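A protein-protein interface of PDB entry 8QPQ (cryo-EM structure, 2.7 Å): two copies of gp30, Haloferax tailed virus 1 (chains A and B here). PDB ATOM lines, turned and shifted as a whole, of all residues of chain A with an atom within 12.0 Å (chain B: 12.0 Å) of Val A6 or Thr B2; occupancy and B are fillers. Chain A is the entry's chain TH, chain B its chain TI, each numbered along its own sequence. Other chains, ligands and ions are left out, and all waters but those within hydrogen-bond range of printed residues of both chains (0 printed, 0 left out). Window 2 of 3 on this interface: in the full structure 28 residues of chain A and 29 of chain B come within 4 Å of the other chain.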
ATOM      1  N   THR A   2       5.597  -0.483   2.474  1.00  0.00           N
ATOM      2  CA  THR A   2       5.375  -1.961   2.315  1.00  0.00           C
ATOM      3  C   THR A   2       5.936  -2.432   0.973  1.00  0.00           C
ATOM      4  O   THR A   2       6.109  -1.638   0.060  1.00  0.00           O
ATOM      5  CB  THR A   2       3.892  -2.337   2.436  1.00  0.00           C
ATOM      6  OG1 THR A   2       3.115  -1.488   1.583  1.00  0.00           O
ATOM      7  CG2 THR A   2       3.359  -2.173   3.846  1.00  0.00           C
ATOM      8  N   ASP A   3       6.185  -3.748   0.872  1.00  0.00           N
ATOM      9  CA  ASP A   3       6.683  -4.399  -0.335  1.00  0.00           C
ATOM     10  C   ASP A   3       5.622  -4.383  -1.443  1.00  0.00           C
ATOM     11  O   ASP A   3       4.470  -4.747  -1.211  1.00  0.00           O
ATOM     12  CB  ASP A   3       7.114  -5.842  -0.026  1.00  0.00           C
ATOM     13  CG  ASP A   3       8.257  -5.996   0.968  1.00  0.00           C
ATOM     14  OD1 ASP A   3       8.720  -4.974   1.515  1.00  0.00           O
ATOM     15  OD2 ASP A   3       8.676  -7.150   1.195  1.00  0.00           O
ATOM     16  N   THR A   4       6.032  -4.071  -2.684  1.00  0.00           N
ATOM     17  CA  THR A   4       5.161  -4.207  -3.849  1.00  0.00           C
ATOM     18  C   THR A   4       5.602  -5.395  -4.702  1.00  0.00           C
ATOM     19  O   THR A   4       6.776  -5.520  -5.039  1.00  0.00           O
ATOM     20  CB  THR A   4       5.115  -2.928  -4.695  1.00  0.00           C
ATOM     21  OG1 THR A   4       4.749  -1.819  -3.879  1.00  0.00           O
ATOM     22  CG2 THR A   4       4.130  -3.004  -5.843  1.00  0.00           C
ATOM     23  N   ILE A   5       4.639  -6.253  -5.064  1.00  0.00           N
ATOM     24  CA  ILE A   5       4.868  -7.397  -5.932  1.00  0.00           C
ATOM     25  C   ILE A   5       3.870  -7.351  -7.089  1.00  0.00           C
ATOM     26  O   ILE A   5       2.718  -6.947  -6.924  1.00  0.00           O
ATOM     27  CB  ILE A   5       4.844  -8.716  -5.117  1.00  0.00           C
ATOM     28  CG1 ILE A   5       6.077  -8.780  -4.207  1.00  0.00           C
ATOM     29  CG2 ILE A   5       4.758  -9.951  -6.008  1.00  0.00           C
ATOM     30  CD1 ILE A   5       6.043  -9.855  -3.132  1.00  0.00           C
ATOM     31  N   VAL A   6       4.329  -7.760  -8.275  1.00  0.00           N
ATOM     32  CA  VAL A   6       3.471  -7.917  -9.441  1.00  0.00           C
ATOM     33  C   VAL A   6       2.961  -9.359  -9.497  1.00  0.00           C
ATOM     34  O   VAL A   6       3.753 -10.301  -9.534  1.00  0.00           O
ATOM     35  CB  VAL A   6       4.210  -7.530 -10.733  1.00  0.00           C
ATOM     36  CG1 VAL A   6       3.401  -7.841 -11.983  1.00  0.00           C
ATOM     37  CG2 VAL A   6       4.625  -6.069 -10.724  1.00  0.00           C
ATOM     38  N   ASN A   7       1.634  -9.511  -9.493  1.00  0.00           N
ATOM     39  CA  ASN A   7       1.015 -10.829  -9.494  1.00  0.00           C
ATOM     40  C   ASN A   7       0.609 -11.220 -10.902  1.00  0.00           C
ATOM     41  O   ASN A   7      -0.352 -10.659 -11.413  1.00  0.00           O
ATOM     42  CB  ASN A   7      -0.236 -10.880  -8.613  1.00  0.00           C
ATOM     43  CG  ASN A   7       0.086 -10.826  -7.129  1.00  0.00           C
ATOM     44  OD1 ASN A   7       1.251 -10.776  -6.697  1.00  0.00           O
ATOM     45  ND2 ASN A   7      -0.959 -10.861  -6.320  1.00  0.00           N
ATOM     46  N   VAL A   8       1.283 -12.213 -11.497  1.00  0.00           N
ATOM     47  CA  VAL A   8       0.806 -12.792 -12.743  1.00  0.00           C
ATOM     48  C   VAL A   8       0.012 -14.052 -12.412  1.00  0.00           C
ATOM     49  O   VAL A   8       0.334 -14.777 -11.481  1.00  0.00           O
ATOM     50  CB  VAL A   8       1.955 -13.023 -13.747  1.00  0.00           C
ATOM     51  CG1 VAL A   8       1.509 -13.797 -14.977  1.00  0.00           C
ATOM     52  CG2 VAL A   8       2.552 -11.688 -14.154  1.00  0.00           C
ATOM     53  N   GLN A   9      -1.047 -14.303 -13.179  1.00  0.00           N
ATOM     54  CA  GLN A   9      -1.985 -15.365 -12.854  1.00  0.00           C
ATOM     55  C   GLN A   9      -1.458 -16.751 -13.229  1.00  0.00           C
ATOM     56  O   GLN A   9      -0.748 -16.923 -14.218  1.00  0.00           O
ATOM     57  CB  GLN A   9      -3.357 -15.047 -13.444  1.00  0.00           C
ATOM     58  CG  GLN A   9      -4.521 -15.528 -12.573  1.00  0.00           C
ATOM     59  CD  GLN A   9      -4.540 -14.903 -11.187  1.00  0.00           C
ATOM     60  OE1 GLN A   9      -3.961 -13.837 -10.947  1.00  0.00           O
ATOM     61  NE2 GLN A   9      -5.137 -15.607 -10.239  1.00  0.00           N
ATOM     62  N   GLY A  10      -1.854 -17.738 -12.412  1.00  0.00           N
ATOM     63  CA  GLY A  10      -1.388 -19.115 -12.413  1.00  0.00           C
ATOM     64  C   GLY A  10      -1.656 -19.873 -13.707  1.00  0.00           C
ATOM     65  O   GLY A  10      -2.428 -19.433 -14.564  1.00  0.00           O
ATOM     66  N   THR B   2       9.926  -4.100 -10.619  1.00  0.00           N
ATOM     67  CA  THR B   2       9.681  -4.671  -9.260  1.00  0.00           C
ATOM     68  C   THR B   2       9.421  -6.172  -9.368  1.00  0.00           C
ATOM     69  O   THR B   2       9.236  -6.708 -10.463  1.00  0.00           O
ATOM     70  CB  THR B   2       8.550  -3.937  -8.529  1.00  0.00           C
ATOM     71  OG1 THR B   2       7.391  -3.907  -9.361  1.00  0.00           O
ATOM     72  CG2 THR B   2       8.926  -2.530  -8.121  1.00  0.00           C
ATOM     73  N   ASP B   3       9.404  -6.859  -8.210  1.00  0.00           N
ATOM     74  CA  ASP B   3       9.380  -8.318  -8.113  1.00  0.00           C
ATOM     75  C   ASP B   3       8.091  -8.927  -8.693  1.00  0.00           C
ATOM     76  O   ASP B   3       6.995  -8.472  -8.395  1.00  0.00           O
ATOM     77  CB  ASP B   3       9.534  -8.784  -6.660  1.00  0.00           C
ATOM     78  CG  ASP B   3      10.826  -8.386  -5.955  1.00  0.00           C
ATOM     79  OD1 ASP B   3      11.517  -7.493  -6.453  1.00  0.00           O
ATOM     80  OD2 ASP B   3      11.127  -8.994  -4.907  1.00  0.00           O
ATOM     81  N   THR B   4       8.240  -9.914  -9.594  1.00  0.00           N
ATOM     82  CA  THR B   4       7.096 -10.565 -10.224  1.00  0.00           C
ATOM     83  C   THR B   4       6.943 -11.985  -9.682  1.00  0.00           C
ATOM     84  O   THR B   4       7.907 -12.757  -9.670  1.00  0.00           O
ATOM     85  CB  THR B   4       7.202 -10.580 -11.757  1.00  0.00           C
ATOM     86  OG1 THR B   4       7.385  -9.248 -12.236  1.00  0.00           O
ATOM     87  CG2 THR B   4       5.991 -11.178 -12.440  1.00  0.00           C
ATOM     88  N   ILE B   5       5.714 -12.327  -9.267  1.00  0.00           N
ATOM     89  CA  ILE B   5       5.391 -13.655  -8.766  1.00  0.00           C
ATOM     90  C   ILE B   5       4.205 -14.216  -9.549  1.00  0.00           C
ATOM     91  O   ILE B   5       3.284 -13.490  -9.915  1.00  0.00           O
ATOM     92  CB  ILE B   5       5.200 -13.641  -7.229  1.00  0.00           C
ATOM     93  CG1 ILE B   5       6.549 -13.376  -6.548  1.00  0.00           C
ATOM     94  CG2 ILE B   5       4.566 -14.928  -6.710  1.00  0.00           C
ATOM     95  CD1 ILE B   5       6.484 -13.050  -5.064  1.00  0.00           C
ATOM     96  N   VAL B   6       4.257 -15.524  -9.824  1.00  0.00           N
ATOM     97  CA  VAL B   6       3.147 -16.239 -10.433  1.00  0.00           C
ATOM     98  C   VAL B   6       2.282 -16.839  -9.326  1.00  0.00           C
ATOM     99  O   VAL B   6       2.760 -17.638  -8.517  1.00  0.00           O
ATOM    100  CB  VAL B   6       3.650 -17.316 -11.412  1.00  0.00           C
ATOM    101  CG1 VAL B   6       2.523 -18.203 -11.929  1.00  0.00           C
ATOM    102  CG2 VAL B   6       4.425 -16.702 -12.567  1.00  0.00           C
ATOM    103  N   ASN B   7       1.002 -16.455  -9.310  1.00  0.00           N
ATOM    104  CA  ASN B   7       0.072 -16.926  -8.291  1.00  0.00           C
ATOM    105  C   ASN B   7      -0.709 -18.127  -8.815  1.00  0.00           C
ATOM    106  O   ASN B   7      -1.569 -17.956  -9.679  1.00  0.00           O
ATOM    107  CB  ASN B   7      -0.956 -15.855  -7.938  1.00  0.00           C
ATOM    108  CG  ASN B   7      -0.395 -14.668  -7.189  1.00  0.00           C
ATOM    109  OD1 ASN B   7       0.779 -14.618  -6.820  1.00  0.00           O
ATOM    110  ND2 ASN B   7      -1.254 -13.701  -6.940  1.00  0.00           N
ATOM    111  N   VAL B   8      -0.449 -19.327  -8.279  1.00  0.00           N
ATOM    112  CA  VAL B   8      -1.303 -20.469  -8.561  1.00  0.00           C
ATOM    113  C   VAL B   8      -2.328 -20.601  -7.437  1.00  0.00           C
ATOM    114  O   VAL B   8      -2.040 -20.319  -6.285  1.00  0.00           O
ATOM    115  CB  VAL B   8      -0.479 -21.752  -8.810  1.00  0.00           C
ATOM    116  CG1 VAL B   8      -1.341 -22.999  -8.907  1.00  0.00           C
ATOM    117  CG2 VAL B   8       0.339 -21.585 -10.078  1.00  0.00           C
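O of Asp B3 lies within hydrogen-bond range of N of Val A6 (2.8 Å).
The backbone carbonyl oxygen (O) of Val A6 lies within hydrogen-bond range of the backbone NH (N) of Ile B5 (2.8 Å).
The side-chain amide nitrogen of Asn A7 sits close to the side-chain amide nitrogen of Asn B7 (2.9 Å).
O of Ile B5 sits at hydrogen-bond distance from N of Val A8, at 2.9 Å.
O of Val A8 lies within hydrogen-bond range of N of Asn B7 (2.8 Å).
The backbone carbonyl oxygen (O) of Asn B7 is in hydrogen-bond range of the backbone NH (N) of Gly A10, at 2.8 Å.
O of Asp B3 touches CA of Ile A5, 3.4 Å away.
Ile A5 touches Ile B5.
Val A6 touches Thr B2 (CG2 to OG1, 3.8 Å).
O of Val A6 touches CA of Thr B4, 3.4 Å away.
Asn A7 touches Ile B5.
Val A8 touches Thr B4.
Val A8 touches Val B6 (O to CA, 3.3 Å).
Gln A9 touches Asn B7 (C to O, 3.8 Å).
Gly A10 touches Val B8.
Val A6 touches just these residues of chain B: Thr B2, Asp B3, Thr B4 and Ile B5.
Of chain B, only Ile B5 (3.5 Å) and Asn B7 (2.9 Å) come within 4 Å of Asn A7.
Printed residues of chain B within 4 Å of Gln A9: Asn B7.
Printed residues of chain B within 4 Å of Gly A10: Asn B7 (2.8 Å) and Val B8 (3.8 Å).
Thr B2 touches just one residue of chain A: Val A6.
Asp B3 touches two residues of chain A.
Thr B4 touches just these residues of chain A: Val A6 and Val A8.
Ile B5 touches just these residues of chain A: Ile A5 (3.7 Å), Val A6 (2.8 Å), Asn A7 (3.5 Å) and Val A8 (2.9 Å).
Of the printed residues of chain A, Val B6 touches Val A8 (3.3 Å).
Of the printed residues of chain A, Val B8 touches Gly A10 (3.8 Å).
The nearest residue of chain B that does not touch Val A6 is Val B6 (5.3 Å).
The nearest residue of chain A that does not touch Thr B2 is Thr A4 (4.2 Å).
Of the 9 printed residues of chain A, 6 touch a printed residue of chain B.
Printed residues of chain A that touch a printed residue of chain B: Ile A5, Val A6, Asn A7, Val A8, Gln A9 and Gly A10.
Hydrophobic or aromatic side chains of chain A within 4 Å of the printed part of chain B: Ile A5, Val A6 and Val A8.
Printed residues of chain B that touch a printed residue of chain A: Thr B2, Asp B3, Thr B4, Ile B5, Val B6, Asn B7 and Val B8.
Hydrophobic or aromatic side chains of chain B within 4 Å of the printed part of chain A: Ile B5 and Val B8.
Among the printed residues, 15 pairs touch across the chains.
Among the printed residues, no Asp or Glu carboxylate lies within 4 Å of a Lys or Arg side-chain nitrogen of the other chain.
Val A6 touches Thr B2, but with the chains exchanged Thr A2 does not touch Val B6 (17.1 Å).
Val A6 touches Asp B3, but with the chains exchanged Asp A3 does not touch Val B6 (13.8 Å).
Val A6 touches Thr B4, but with the chains exchanged Thr A4 does not touch Val B6 (11.4 Å).
Asn A7 touches Ile B5, but with the chains exchanged Ile A5 does not touch Asn B7 (6.2 Å).
Positions printed for both chains: 2, 3, 4, 5, 6, 7 and 8.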
